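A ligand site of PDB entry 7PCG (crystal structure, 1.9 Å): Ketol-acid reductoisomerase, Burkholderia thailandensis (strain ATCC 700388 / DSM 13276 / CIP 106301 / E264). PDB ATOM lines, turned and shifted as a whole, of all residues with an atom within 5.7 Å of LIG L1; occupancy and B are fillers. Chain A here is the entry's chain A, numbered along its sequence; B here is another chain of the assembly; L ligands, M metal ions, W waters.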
ATOM      1  N   ILE A  29      18.681   9.965 -28.594  1.00  0.00           N
ATOM      2  CA  ILE A  29      19.275   9.845 -27.232  1.00  0.00           C
ATOM      3  C   ILE A  29      20.284   8.688 -27.266  1.00  0.00           C
ATOM      4  O   ILE A  29      19.846   7.520 -27.391  1.00  0.00           O
ATOM      5  CB  ILE A  29      18.192   9.638 -26.156  1.00  0.00           C
ATOM      6  CG1 ILE A  29      17.102  10.714 -26.248  1.00  0.00           C
ATOM      7  CG2 ILE A  29      18.808   9.580 -24.762  1.00  0.00           C
ATOM      8  CD1 ILE A  29      17.623  12.144 -26.252  1.00  0.00           C
ATOM      9  N   GLY A  30      21.565   9.010 -27.168  1.00  0.00           N
ATOM     10  CA  GLY A  30      22.679   8.061 -27.373  1.00  0.00           C
ATOM     11  C   GLY A  30      23.190   8.131 -28.801  1.00  0.00           C
ATOM     12  O   GLY A  30      22.384   8.395 -29.705  1.00  0.00           O
ATOM     13  N   TYR A  31      24.493   7.927 -28.992  1.00  0.00           N
ATOM     14  CA  TYR A  31      25.191   8.004 -30.297  1.00  0.00           C
ATOM     15  C   TYR A  31      26.118   6.800 -30.419  1.00  0.00           C
ATOM     16  O   TYR A  31      27.228   6.938 -30.977  1.00  0.00           O
ATOM     17  CB  TYR A  31      25.902   9.357 -30.401  1.00  0.00           C
ATOM     18  CG  TYR A  31      26.263   9.772 -31.806  1.00  0.00           C
ATOM     19  CD1 TYR A  31      25.292  10.240 -32.690  1.00  0.00           C
ATOM     20  CD2 TYR A  31      27.572   9.700 -32.263  1.00  0.00           C
ATOM     21  CE1 TYR A  31      25.618  10.626 -33.982  1.00  0.00           C
ATOM     22  CE2 TYR A  31      27.907  10.078 -33.547  1.00  0.00           C
ATOM     23  CZ  TYR A  31      26.930  10.552 -34.409  1.00  0.00           C
ATOM     24  OH  TYR A  31      27.272  10.915 -35.677  1.00  0.00           O
ATOM     25  N   GLY A  32      25.656   5.659 -29.907  1.00  0.00           N
ATOM     26  CA  GLY A  32      26.372   4.361 -29.946  1.00  0.00           C
ATOM     27  C   GLY A  32      26.108   3.626 -31.241  1.00  0.00           C
ATOM     28  O   GLY A  32      25.907   4.282 -32.283  1.00  0.00           O
ATOM     29  N   ILE A  33      26.094   2.295 -31.180  1.00  0.00           N
ATOM     30  CA  ILE A  33      25.952   1.388 -32.359  1.00  0.00           C
ATOM     31  C   ILE A  33      24.690   1.786 -33.132  1.00  0.00           C
ATOM     32  O   ILE A  33      24.802   2.008 -34.362  1.00  0.00           O
ATOM     33  CB  ILE A  33      25.945  -0.090 -31.908  1.00  0.00           C
ATOM     34  CG1 ILE A  33      27.292  -0.481 -31.282  1.00  0.00           C
ATOM     35  CG2 ILE A  33      25.580  -1.023 -33.052  1.00  0.00           C
ATOM     36  CD1 ILE A  33      27.174  -1.376 -30.069  1.00  0.00           C
ATOM     37  N   GLN A  34      23.546   1.907 -32.459  1.00  0.00           N
ATOM     38  CA  GLN A  34      22.234   2.236 -33.089  1.00  0.00           C
ATOM     39  C   GLN A  34      22.105   3.754 -33.270  1.00  0.00           C
ATOM     40  O   GLN A  34      21.764   4.182 -34.391  1.00  0.00           O
ATOM     41  CB  GLN A  34      21.086   1.660 -32.260  1.00  0.00           C
ATOM     42  CG  GLN A  34      20.969   0.149 -32.353  1.00  0.00           C
ATOM     43  CD  GLN A  34      20.626  -0.334 -33.741  1.00  0.00           C
ATOM     44  OE1 GLN A  34      19.849   0.302 -34.465  1.00  0.00           O
ATOM     45  NE2 GLN A  34      21.193  -1.459 -34.136  1.00  0.00           N
ATOM     46  N   GLY A  35      22.371   4.525 -32.211  1.00  0.00           N
ATOM     47  CA  GLY A  35      22.207   5.999 -32.186  1.00  0.00           C
ATOM     48  C   GLY A  35      22.871   6.677 -33.378  1.00  0.00           C
ATOM     49  O   GLY A  35      22.205   7.513 -34.032  1.00  0.00           O
ATOM     50  N   ASN A  53      23.163  13.304 -25.228  1.00  0.00           N
ATOM     51  CA  ASN A  53      24.211  12.351 -24.794  1.00  0.00           C
ATOM     52  C   ASN A  53      24.863  12.848 -23.502  1.00  0.00           C
ATOM     53  O   ASN A  53      24.990  14.084 -23.326  1.00  0.00           O
ATOM     54  CB  ASN A  53      25.227  12.119 -25.919  1.00  0.00           C
ATOM     55  CG  ASN A  53      25.947  10.789 -25.793  1.00  0.00           C
ATOM     56  OD1 ASN A  53      25.524   9.793 -26.366  1.00  0.00           O
ATOM     57  ND2 ASN A  53      27.036  10.774 -25.037  1.00  0.00           N
ATOM     58  N   ILE A  54      25.246  11.914 -22.629  1.00  0.00           N
ATOM     59  CA  ILE A  54      26.055  12.182 -21.406  1.00  0.00           C
ATOM     60  C   ILE A  54      27.468  12.582 -21.846  1.00  0.00           C
ATOM     61  O   ILE A  54      27.771  12.471 -23.058  1.00  0.00           O
ATOM     62  CB  ILE A  54      26.067  10.969 -20.450  1.00  0.00           C
ATOM     63  CG1 ILE A  54      26.636   9.705 -21.101  1.00  0.00           C
ATOM     64  CG2 ILE A  54      24.679  10.724 -19.868  1.00  0.00           C
ATOM     65  CD1 ILE A  54      27.067   8.652 -20.110  1.00  0.00           C
ATOM     66  N   ASP A  56      30.716  11.845 -22.480  1.00  0.00           N
ATOM     67  CA  ASP A  56      31.647  10.718 -22.806  1.00  0.00           C
ATOM     68  C   ASP A  56      32.104  10.844 -24.270  1.00  0.00           C
ATOM     69  O   ASP A  56      31.786  11.879 -24.903  1.00  0.00           O
ATOM     70  CB  ASP A  56      31.019   9.369 -22.479  1.00  0.00           C
ATOM     71  CG  ASP A  56      29.781   9.033 -23.303  1.00  0.00           C
ATOM     72  OD1 ASP A  56      29.557   9.688 -24.336  1.00  0.00           O
ATOM     73  OD2 ASP A  56      29.039   8.113 -22.896  1.00  0.00           O
ATOM     74  N   TYR A  58      31.219   9.505 -27.026  1.00  0.00           N
ATOM     75  CA  TYR A  58      30.100   9.526 -28.014  1.00  0.00           C
ATOM     76  C   TYR A  58      29.623  10.966 -28.229  1.00  0.00           C
ATOM     77  O   TYR A  58      29.302  11.312 -29.381  1.00  0.00           O
ATOM     78  CB  TYR A  58      28.965   8.599 -27.551  1.00  0.00           C
ATOM     79  CG  TYR A  58      29.347   7.152 -27.409  1.00  0.00           C
ATOM     80  CD1 TYR A  58      29.694   6.625 -26.171  1.00  0.00           C
ATOM     81  CD2 TYR A  58      29.347   6.296 -28.501  1.00  0.00           C
ATOM     82  CE1 TYR A  58      30.041   5.290 -26.028  1.00  0.00           C
ATOM     83  CE2 TYR A  58      29.688   4.962 -28.374  1.00  0.00           C
ATOM     84  CZ  TYR A  58      30.033   4.455 -27.127  1.00  0.00           C
ATOM     85  OH  TYR A  58      30.366   3.137 -27.015  1.00  0.00           O
ATOM     86  N   ILE A  72      20.919  15.084 -22.321  1.00  0.00           N
ATOM     87  CA  ILE A  72      19.682  14.345 -22.733  1.00  0.00           C
ATOM     88  C   ILE A  72      18.457  15.222 -22.478  1.00  0.00           C
ATOM     89  O   ILE A  72      17.616  15.329 -23.389  1.00  0.00           O
ATOM     90  CB  ILE A  72      19.615  12.968 -22.033  1.00  0.00           C
ATOM     91  CG1 ILE A  72      20.757  12.067 -22.504  1.00  0.00           C
ATOM     92  CG2 ILE A  72      18.256  12.316 -22.240  1.00  0.00           C
ATOM     93  CD1 ILE A  72      20.914  10.780 -21.717  1.00  0.00           C
ATOM     94  N   LEU A  84      15.199   6.513 -27.763  1.00  0.00           N
ATOM     95  CA  LEU A  84      16.004   6.137 -26.569  1.00  0.00           C
ATOM     96  C   LEU A  84      16.958   5.001 -26.949  1.00  0.00           C
ATOM     97  O   LEU A  84      16.574   3.815 -26.772  1.00  0.00           O
ATOM     98  CB  LEU A  84      15.075   5.741 -25.422  1.00  0.00           C
ATOM     99  CG  LEU A  84      15.752   5.463 -24.089  1.00  0.00           C
ATOM    100  CD1 LEU A  84      16.705   6.588 -23.698  1.00  0.00           C
ATOM    101  CD2 LEU A  84      14.725   5.243 -22.987  1.00  0.00           C
ATOM    102  N   LEU A  85      18.134   5.346 -27.469  1.00  0.00           N
ATOM    103  CA  LEU A  85      19.146   4.384 -27.989  1.00  0.00           C
ATOM    104  C   LEU A  85      20.380   4.387 -27.061  1.00  0.00           C
ATOM    105  O   LEU A  85      21.503   4.697 -27.523  1.00  0.00           O
ATOM    106  CB  LEU A  85      19.477   4.759 -29.434  1.00  0.00           C
ATOM    107  CG  LEU A  85      18.266   4.780 -30.377  1.00  0.00           C
ATOM    108  CD1 LEU A  85      18.668   5.205 -31.780  1.00  0.00           C
ATOM    109  CD2 LEU A  85      17.568   3.424 -30.416  1.00  0.00           C
ATOM    110  N   ILE A  86      20.151   4.043 -25.794  1.00  0.00           N
ATOM    111  CA  ILE A  86      21.202   3.824 -24.757  1.00  0.00           C
ATOM    112  C   ILE A  86      20.989   2.420 -24.180  1.00  0.00           C
ATOM    113  O   ILE A  86      19.939   1.826 -24.399  1.00  0.00           O
ATOM    114  CB  ILE A  86      21.125   4.933 -23.678  1.00  0.00           C
ATOM    115  CG1 ILE A  86      19.824   4.883 -22.880  1.00  0.00           C
ATOM    116  CG2 ILE A  86      21.362   6.299 -24.311  1.00  0.00           C
ATOM    117  CD1 ILE A  86      19.797   5.795 -21.681  1.00  0.00           C
ATOM    118  N   PRO A  87      21.983   1.844 -23.467  1.00  0.00           N
ATOM    119  CA  PRO A  87      21.819   0.525 -22.843  1.00  0.00           C
ATOM    120  C   PRO A  87      20.561   0.422 -21.959  1.00  0.00           C
ATOM    121  O   PRO A  87      20.219   1.391 -21.315  1.00  0.00           O
ATOM    122  CB  PRO A  87      23.087   0.371 -21.999  1.00  0.00           C
ATOM    123  CG  PRO A  87      24.113   1.206 -22.734  1.00  0.00           C
ATOM    124  CD  PRO A  87      23.334   2.396 -23.255  1.00  0.00           C
ATOM    125  N   ASP A  88      19.951  -0.770 -21.958  1.00  0.00           N
ATOM    126  CA  ASP A  88      18.576  -1.018 -21.439  1.00  0.00           C
ATOM    127  C   ASP A  88      18.510  -0.766 -19.936  1.00  0.00           C
ATOM    128  O   ASP A  88      17.474  -0.257 -19.471  1.00  0.00           O
ATOM    129  CB  ASP A  88      18.116  -2.424 -21.835  1.00  0.00           C
ATOM    130  CG  ASP A  88      18.059  -2.624 -23.346  1.00  0.00           C
ATOM    131  OD1 ASP A  88      17.203  -1.989 -23.994  1.00  0.00           O
ATOM    132  OD2 ASP A  88      18.899  -3.395 -23.862  1.00  0.00           O
ATOM    133  N   ALA A  90      20.033   1.447 -18.240  1.00  0.00           N
ATOM    134  CA  ALA A  90      20.104   2.919 -18.030  1.00  0.00           C
ATOM    135  C   ALA A  90      18.762   3.588 -18.357  1.00  0.00           C
ATOM    136  O   ALA A  90      18.631   4.788 -18.039  1.00  0.00           O
ATOM    137  CB  ALA A  90      21.219   3.494 -18.852  1.00  0.00           C
ATOM    138  N   HIS A  91      17.816   2.869 -18.969  1.00  0.00           N
ATOM    139  CA  HIS A  91      16.491   3.410 -19.396  1.00  0.00           C
ATOM    140  C   HIS A  91      15.745   4.005 -18.197  1.00  0.00           C
ATOM    141  O   HIS A  91      15.293   5.162 -18.305  1.00  0.00           O
ATOM    142  CB  HIS A  91      15.664   2.328 -20.119  1.00  0.00           C
ATOM    143  CG  HIS A  91      16.069   2.108 -21.535  1.00  0.00           C
ATOM    144  ND1 HIS A  91      15.177   1.728 -22.517  1.00  0.00           N
ATOM    145  CD2 HIS A  91      17.265   2.233 -22.155  1.00  0.00           C
ATOM    146  CE1 HIS A  91      15.804   1.606 -23.663  1.00  0.00           C
ATOM    147  NE2 HIS A  91      17.085   1.915 -23.471  1.00  0.00           N
ATOM    148  N   VAL A  94      17.232   7.438 -16.734  1.00  0.00           N
ATOM    149  CA  VAL A  94      17.192   8.473 -17.812  1.00  0.00           C
ATOM    150  C   VAL A  94      15.723   8.842 -18.082  1.00  0.00           C
ATOM    151  O   VAL A  94      15.432  10.044 -18.229  1.00  0.00           O
ATOM    152  CB  VAL A  94      17.911   8.003 -19.089  1.00  0.00           C
ATOM    153  CG1 VAL A  94      17.673   8.937 -20.278  1.00  0.00           C
ATOM    154  CG2 VAL A  94      19.401   7.829 -18.850  1.00  0.00           C
ATOM    155  N   ALA A 112      14.238   0.710 -28.962  1.00  0.00           N
ATOM    156  CA  ALA A 112      14.677  -0.212 -30.031  1.00  0.00           C
ATOM    157  C   ALA A 112      14.745  -1.656 -29.509  1.00  0.00           C
ATOM    158  O   ALA A 112      15.285  -2.520 -30.224  1.00  0.00           O
ATOM    159  CB  ALA A 112      16.003   0.256 -30.595  1.00  0.00           C
ATOM    160  N   HIS A 113      14.155  -1.903 -28.339  1.00  0.00           N
ATOM    161  CA  HIS A 113      14.155  -3.214 -27.626  1.00  0.00           C
ATOM    162  C   HIS A 113      13.098  -3.138 -26.523  1.00  0.00           C
ATOM    163  O   HIS A 113      13.018  -2.086 -25.871  1.00  0.00           O
ATOM    164  CB  HIS A 113      15.570  -3.529 -27.132  1.00  0.00           C
ATOM    165  CG  HIS A 113      15.733  -4.858 -26.456  1.00  0.00           C
ATOM    166  ND1 HIS A 113      15.272  -6.034 -27.016  1.00  0.00           N
ATOM    167  CD2 HIS A 113      16.350  -5.197 -25.302  1.00  0.00           C
ATOM    168  CE1 HIS A 113      15.579  -7.038 -26.209  1.00  0.00           C
ATOM    169  NE2 HIS A 113      16.247  -6.552 -25.161  1.00  0.00           N
ATOM    170  N   ALA A 134      12.381  -1.778 -33.453  1.00  0.00           N
ATOM    171  CA  ALA A 134      13.524  -2.644 -33.086  1.00  0.00           C
ATOM    172  C   ALA A 134      14.181  -3.196 -34.346  1.00  0.00           C
ATOM    173  O   ALA A 134      13.668  -4.152 -34.937  1.00  0.00           O
ATOM    174  CB  ALA A 134      13.041  -3.749 -32.176  1.00  0.00           C
ATOM    175  N   PRO A 135      15.316  -2.623 -34.807  1.00  0.00           N
ATOM    176  CA  PRO A 135      16.021  -3.144 -35.974  1.00  0.00           C
ATOM    177  C   PRO A 135      16.541  -4.570 -35.719  1.00  0.00           C
ATOM    178  O   PRO A 135      16.864  -4.865 -34.585  1.00  0.00           O
ATOM    179  CB  PRO A 135      17.190  -2.168 -36.185  1.00  0.00           C
ATOM    180  CG  PRO A 135      16.789  -0.925 -35.416  1.00  0.00           C
ATOM    181  CD  PRO A 135      15.973  -1.431 -34.252  1.00  0.00           C
ATOM    182  N   MET A 137      19.283  -5.798 -36.986  1.00  0.00           N
ATOM    183  CA  MET A 137      20.656  -5.627 -37.533  1.00  0.00           C
ATOM    184  C   MET A 137      21.393  -4.593 -36.682  1.00  0.00           C
ATOM    185  O   MET A 137      20.709  -3.752 -36.052  1.00  0.00           O
ATOM    186  CB  MET A 137      20.576  -5.143 -38.990  1.00  0.00           C
ATOM    187  CG  MET A 137      21.910  -5.076 -39.714  1.00  0.00           C
ATOM    188  SD  MET A 137      22.807  -6.643 -39.740  1.00  0.00           S
ATOM    189  CE  MET A 137      21.716  -7.640 -40.756  1.00  0.00           C
ATOM    190  N   TYR A 138      22.729  -4.655 -36.637  1.00  0.00           N
ATOM    191  CA  TYR A 138      23.577  -3.671 -35.902  1.00  0.00           C
ATOM    192  C   TYR A 138      23.911  -2.515 -36.842  1.00  0.00           C
ATOM    193  O   TYR A 138      23.492  -2.534 -38.008  1.00  0.00           O
ATOM    194  CB  TYR A 138      24.765  -4.357 -35.219  1.00  0.00           C
ATOM    195  CG  TYR A 138      25.642  -5.268 -36.050  1.00  0.00           C
ATOM    196  CD1 TYR A 138      26.784  -4.798 -36.663  1.00  0.00           C
ATOM    197  CD2 TYR A 138      25.364  -6.624 -36.131  1.00  0.00           C
ATOM    198  CE1 TYR A 138      27.614  -5.641 -37.390  1.00  0.00           C
ATOM    199  CE2 TYR A 138      26.175  -7.481 -36.864  1.00  0.00           C
ATOM    200  CZ  TYR A 138      27.308  -6.990 -37.484  1.00  0.00           C
ATOM    201  OH  TYR A 138      28.113  -7.827 -38.195  1.00  0.00           O
ATOM    202  N   GLY A 139      24.622  -1.502 -36.318  1.00  0.00           N
ATOM    203  CA  GLY A 139      24.706  -0.135 -36.869  1.00  0.00           C
ATOM    204  C   GLY A 139      25.369  -0.069 -38.241  1.00  0.00           C
ATOM    205  O   GLY A 139      24.741   0.488 -39.155  1.00  0.00           O
ATOM    206  N   ASP A 196      14.825 -11.604 -29.010  1.00  0.00           N
ATOM    207  CA  ASP A 196      16.105 -10.887 -29.180  1.00  0.00           C
ATOM    208  C   ASP A 196      17.164 -11.496 -28.259  1.00  0.00           C
ATOM    209  O   ASP A 196      18.279 -11.781 -28.740  1.00  0.00           O
ATOM    210  CB  ASP A 196      15.926  -9.395 -28.916  1.00  0.00           C
ATOM    211  CG  ASP A 196      17.039  -8.538 -29.498  1.00  0.00           C
ATOM    212  OD1 ASP A 196      17.158  -8.507 -30.734  1.00  0.00           O
ATOM    213  OD2 ASP A 196      17.782  -7.933 -28.700  1.00  0.00           O
ATOM    214  N   GLU B 237      21.759 -11.112 -39.939  1.00  0.00           N
ATOM    215  CA  GLU B 237      22.509 -10.610 -38.762  1.00  0.00           C
ATOM    216  C   GLU B 237      23.551 -11.655 -38.329  1.00  0.00           C
ATOM    217  O   GLU B 237      24.706 -11.262 -38.094  1.00  0.00           O
ATOM    218  CB  GLU B 237      21.576 -10.262 -37.609  1.00  0.00           C
ATOM    219  CG  GLU B 237      22.283  -9.494 -36.502  1.00  0.00           C
ATOM    220  CD  GLU B 237      21.381  -8.934 -35.420  1.00  0.00           C
ATOM    221  OE1 GLU B 237      20.396  -9.621 -35.065  1.00  0.00           O
ATOM    222  OE2 GLU B 237      21.666  -7.833 -34.935  1.00  0.00           O
ATOM    223  N   GLN B 257      30.057  -4.412 -31.575  1.00  0.00           N
ATOM    224  CA  GLN B 257      28.730  -4.197 -32.217  1.00  0.00           C
ATOM    225  C   GLN B 257      27.571  -4.561 -31.280  1.00  0.00           C
ATOM    226  O   GLN B 257      26.419  -4.230 -31.626  1.00  0.00           O
ATOM    227  CB  GLN B 257      28.619  -5.046 -33.493  1.00  0.00           C
ATOM    228  CG  GLN B 257      29.699  -4.735 -34.525  1.00  0.00           C
ATOM    229  CD  GLN B 257      29.543  -3.374 -35.146  1.00  0.00           C
ATOM    230  OE1 GLN B 257      28.799  -2.526 -34.661  1.00  0.00           O
ATOM    231  NE2 GLN B 257      30.240  -3.148 -36.243  1.00  0.00           N
ATOM    232  N   GLY B 258      27.838  -5.241 -30.159  1.00  0.00           N
ATOM    233  CA  GLY B 258      26.806  -5.720 -29.224  1.00  0.00           C
ATOM    234  C   GLY B 258      26.477  -4.686 -28.157  1.00  0.00           C
ATOM    235  O   GLY B 258      27.418  -4.077 -27.597  1.00  0.00           O
ATOM    236  N   SER B 259      25.183  -4.482 -27.868  1.00  0.00           N
ATOM    237  CA  SER B 259      24.694  -3.724 -26.692  1.00  0.00           C
ATOM    238  C   SER B 259      25.225  -4.394 -25.430  1.00  0.00           C
ATOM    239  O   SER B 259      25.566  -5.583 -25.459  1.00  0.00           O
ATOM    240  CB  SER B 259      23.188  -3.646 -26.673  1.00  0.00           C
ATOM    241  OG  SER B 259      22.625  -4.924 -26.420  1.00  0.00           O
ATOM    242  N   PRO B 260      25.350  -3.685 -24.285  1.00  0.00           N
ATOM    243  CA  PRO B 260      25.760  -4.331 -23.035  1.00  0.00           C
ATOM    244  C   PRO B 260      24.874  -5.538 -22.682  1.00  0.00           C
ATOM    245  O   PRO B 260      25.423  -6.534 -22.256  1.00  0.00           O
ATOM    246  CB  PRO B 260      25.641  -3.200 -22.000  1.00  0.00           C
ATOM    247  CG  PRO B 260      25.854  -1.942 -22.828  1.00  0.00           C
ATOM    248  CD  PRO B 260      25.137  -2.243 -24.135  1.00  0.00           C
ATOM    249  N   THR B 261      23.561  -5.422 -22.878  1.00  0.00           N
ATOM    250  CA  THR B 261      22.570  -6.518 -22.665  1.00  0.00           C
ATOM    251  C   THR B 261      22.979  -7.744 -23.474  1.00  0.00           C
ATOM    252  O   THR B 261      23.016  -8.851 -22.904  1.00  0.00           O
ATOM    253  CB  THR B 261      21.152  -6.056 -23.032  1.00  0.00           C
ATOM    254  OG1 THR B 261      20.792  -4.997 -22.144  1.00  0.00           O
ATOM    255  CG2 THR B 261      20.120  -7.152 -22.951  1.00  0.00           C
HETATM  256  P1  LIG L   1      25.819   1.178 -26.980  1.00  0.00           P
HETATM  257  O1  LIG L   1      26.601   0.342 -26.023  1.00  0.00           O
HETATM  258  O2  LIG L   1      26.424   1.487 -28.309  1.00  0.00           O
HETATM  259  O3  LIG L   1      25.364   2.527 -26.252  1.00  0.00           O
HETATM  260  C1  LIG L   1      26.295   3.633 -26.122  1.00  0.00           C
HETATM  261  C2  LIG L   1      25.509   4.908 -25.998  1.00  0.00           C
HETATM  262  O4  LIG L   1      24.761   4.896 -24.752  1.00  0.00           O
HETATM  263  C3  LIG L   1      26.334   6.200 -25.965  1.00  0.00           C
HETATM  264  O5  LIG L   1      25.659   7.236 -26.650  1.00  0.00           O
HETATM  265  C4  LIG L   1      26.482   6.460 -24.457  1.00  0.00           C
HETATM  266  O6  LIG L   1      26.733   7.822 -24.171  1.00  0.00           O
HETATM  267  C5  LIG L   1      25.100   6.016 -23.969  1.00  0.00           C
HETATM  268  N1  LIG L   1      25.056   5.615 -22.563  1.00  0.00           N
HETATM  269  C6  LIG L   1      25.685   4.549 -21.986  1.00  0.00           C
HETATM  270  N2  LIG L   1      25.425   4.422 -20.703  1.00  0.00           N
HETATM  271  C7  LIG L   1      24.568   5.471 -20.424  1.00  0.00           C
HETATM  272  C8  LIG L   1      23.933   5.894 -19.234  1.00  0.00           C
HETATM  273  N3  LIG L   1      24.063   5.276 -18.067  1.00  0.00           N
HETATM  274  N4  LIG L   1      23.134   6.982 -19.302  1.00  0.00           N
HETATM  275  C9  LIG L   1      23.005   7.608 -20.476  1.00  0.00           C
HETATM  276  N5  LIG L   1      23.544   7.308 -21.664  1.00  0.00           N
HETATM  277  C10 LIG L   1      24.325   6.224 -21.563  1.00  0.00           C
HETATM  278  O7  LIG L   1      24.389   0.487 -27.185  1.00  0.00           O
HETATM  279  P2  LIG L   1      23.489   0.089 -28.438  1.00  0.00           P
HETATM  280  O8  LIG L   1      23.953  -1.239 -28.938  1.00  0.00           O
HETATM  281  O9  LIG L   1      23.440   1.230 -29.408  1.00  0.00           O
HETATM  282  O10 LIG L   1      22.059  -0.095 -27.731  1.00  0.00           O
HETATM  283  C11 LIG L   1      21.120   0.994 -27.591  1.00  0.00           C
HETATM  284  C12 LIG L   1      19.717   0.435 -27.619  1.00  0.00           C
HETATM  285  O11 LIG L   1      19.488  -0.157 -28.910  1.00  0.00           O
HETATM  286  C13 LIG L   1      19.392  -0.664 -26.593  1.00  0.00           C
HETATM  287  O12 LIG L   1      18.073  -0.531 -26.098  1.00  0.00           O
HETATM  288  C14 LIG L   1      19.569  -1.941 -27.415  1.00  0.00           C
HETATM  289  O13 LIG L   1      18.827  -3.032 -26.898  1.00  0.00           O
HETATM  290  C15 LIG L   1      19.023  -1.486 -28.762  1.00  0.00           C
HETATM  291  N6  LIG L   1      19.499  -2.302 -29.917  1.00  0.00           N
HETATM  292  C16 LIG L   1      20.859  -2.412 -30.191  1.00  0.00           C
HETATM  293  C17 LIG L   1      21.279  -3.075 -31.346  1.00  0.00           C
HETATM  294  C18 LIG L   1      22.749  -3.135 -31.664  1.00  0.00           C
HETATM  295  O14 LIG L   1      23.105  -3.224 -32.840  1.00  0.00           O
HETATM  296  N7  LIG L   1      23.617  -3.104 -30.664  1.00  0.00           N
HETATM  297  C19 LIG L   1      20.329  -3.652 -32.182  1.00  0.00           C
HETATM  298  C20 LIG L   1      18.991  -3.490 -31.921  1.00  0.00           C
HETATM  299  C21 LIG L   1      18.604  -2.936 -30.716  1.00  0.00           C
HETATM  300  C1  LG2 L   2      22.379  -6.085 -29.700  1.00  0.00           C
HETATM  301  C2  LG2 L   2      22.108  -6.627 -31.127  1.00  0.00           C
HETATM  302  C3  LG2 L   2      20.620  -6.795 -31.552  1.00  0.00           C
HETATM  303  C4  LG2 L   2      23.084  -6.357 -32.149  1.00  0.00           C
HETATM  304  C5  LG2 L   2      22.993  -7.641 -31.579  1.00  0.00           C
HETATM  305  O1  LG2 L   2      21.430  -5.985 -28.890  1.00  0.00           O
HETATM  306  O2  LG2 L   2      20.371  -6.930 -32.775  1.00  0.00           O
HETATM  307  O3  LG2 L   2      19.755  -6.825 -30.645  1.00  0.00           O
HETATM  308  O4  LG2 L   2      23.562  -5.807 -29.438  1.00  0.00           O
HETATM  309 MG    MG M   1      19.517  -7.036 -28.600  1.00  0.00          MG
HETATM  310 MG    MG M   2      18.496  -8.257 -32.163  1.00  0.00          MG
HETATM  311  O   HOH W   1      22.635   9.128 -17.686  1.00  0.00           O
HETATM  312  O   HOH W   2      18.379  -5.131 -28.595  1.00  0.00           O
HETATM  313  O   HOH W   3      17.343  -6.485 -32.521  1.00  0.00           O
HETATM  314  O   HOH W   4      27.986  -1.721 -26.369  1.00  0.00           O
HETATM  315  O   HOH W   5      16.139  -5.081 -30.155  1.00  0.00           O
HETATM  316  O   HOH W   6      24.162   9.333 -23.504  1.00  0.00           O
HETATM  317  O   HOH W   7      25.456   1.837 -19.463  1.00  0.00           O
HETATM  318  O   HOH W   8      29.111   1.655 -28.856  1.00  0.00           O
HETATM  319  O   HOH W   9      16.107   1.196 -26.979  1.00  0.00           O
HETATM  320  O   HOH W  10      23.296   4.062 -29.520  1.00  0.00           O
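A nitrogen (N7) of LIG L1 is in hydrogen-bond range of an oxygen (O4) of LG2 L2.
An oxygen (O4) of LG2 L2 lies within hydrogen-bond range of the side-chain hydroxyl (OG) of Ser 259 of chain B (3.3 Å). N of Tyr 31 is in hydrogen-bond range of O5 of LIG L1 (2.7 Å). O2 of LIG L1 sits at hydrogen-bond distance from N of Ile 33 (3.0 Å). An oxygen (O14) of LIG L1 sits at hydrogen-bond distance from the side-chain amide nitrogen of Gln 34 (2.9 Å). An oxygen (O4) of LG2 L2 sits at hydrogen-bond distance from the backbone NH (N) of Ser 259 of chain B, at 2.6 Å. O of Gln 257 of chain B lies within hydrogen-bond range of N7 of LIG L1 (3.2 Å). The backbone NH (N) of Gln 34 sits at hydrogen-bond distance from an oxygen (O9) of LIG L1 (3.1 Å). O6 of LIG L1 sits at hydrogen-bond distance from OD2 of Asp 56 (2.7 Å). The side-chain carboxylate (OE2) of Glu 237 of chain B lies close to an oxygen (O2) of LG2 L2, at 2.7 Å. O of Ile 86 sits close to O12 of LIG L1 (3.5 Å). OD1 of Asp 88 is in hydrogen-bond range of O12 of LIG L1, at 2.7 Å. The side-chain amide oxygen (OD1) of Asn 53 lies within hydrogen-bond range of an oxygen (O5) of LIG L1 (2.6 Å).
Water W4 bridges O1 of LIG L1 (2.5 Å) and O of Gly 258 of chain B (2.7 Å). Water W8 bridges OH of Tyr 58 and O2 of LIG L1. Water W9 lies within hydrogen-bond range of O of Leu 84 (2.7 Å), O12 of LIG L1 (2.8 Å) and N of Ala 112 (2.8 Å). Water W6 lies within hydrogen-bond range of a nitrogen (N5) of LIG L1 (2.8 Å), the backbone NH of Ile 54 (2.9 Å) and the side-chain amide oxygen of Asn 53 (3.2 Å). Water W10 lies within hydrogen-bond range of O of Leu 85 (2.8 Å), O9 of LIG L1 (2.8 Å), N of Gly 32 (2.9 Å) and N of Gly 35 (2.9 Å). Water W5 bridges O of Ala 112 (2.7 Å) and ND1 of His 113 (3.4 Å).
NE2 of Gln 34 lies within hydrogen-bond range of O of Met 137 (3.0 Å). The backbone carbonyl oxygen (O) of Ile 86 is in hydrogen-bond range of a ring nitrogen (NE2) of His 91. The backbone carbonyl oxygen (O) of Ile 29 sits at hydrogen-bond distance from the backbone NH (N) of Leu 85, at 2.8 Å. The side-chain amide oxygen (OD1) of Asn 53 sits at hydrogen-bond distance from the backbone NH (N) of Tyr 31. The side-chain carboxylate (OD2) of Asp 88 is in hydrogen-bond range of the side-chain hydroxyl (OG1) of Thr 261 of chain B, at 3.0 Å. N of Tyr 58 is in hydrogen-bond range of OD1 of Asp 56. The side-chain amide nitrogen of Asn 53 lies within hydrogen-bond range of the side-chain carboxylate of Asp 56 (2.8 Å).
N7 of LIG L1 lies close to N of Ser 259 of chain B (3.5 Å). Residues that only touch LIG L1: Gly 30, Gly 32, Ile 54, Tyr 58, Ile 72, Leu 85, Pro 87, Ala 90, His 91, Val 94, Ala 112, His 113, Pro 135, Met 137, Tyr 138 and Pro 260 of chain B. Hydrophobic or aromatic side chains that line LIG L1: Ile 33, Ile 54, Tyr 58, Ile 72, Ile 86, Pro 87, Ala 90, His 91, Val 94, Ala 112, His 113, Tyr 138 and Pro 260 of chain B.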
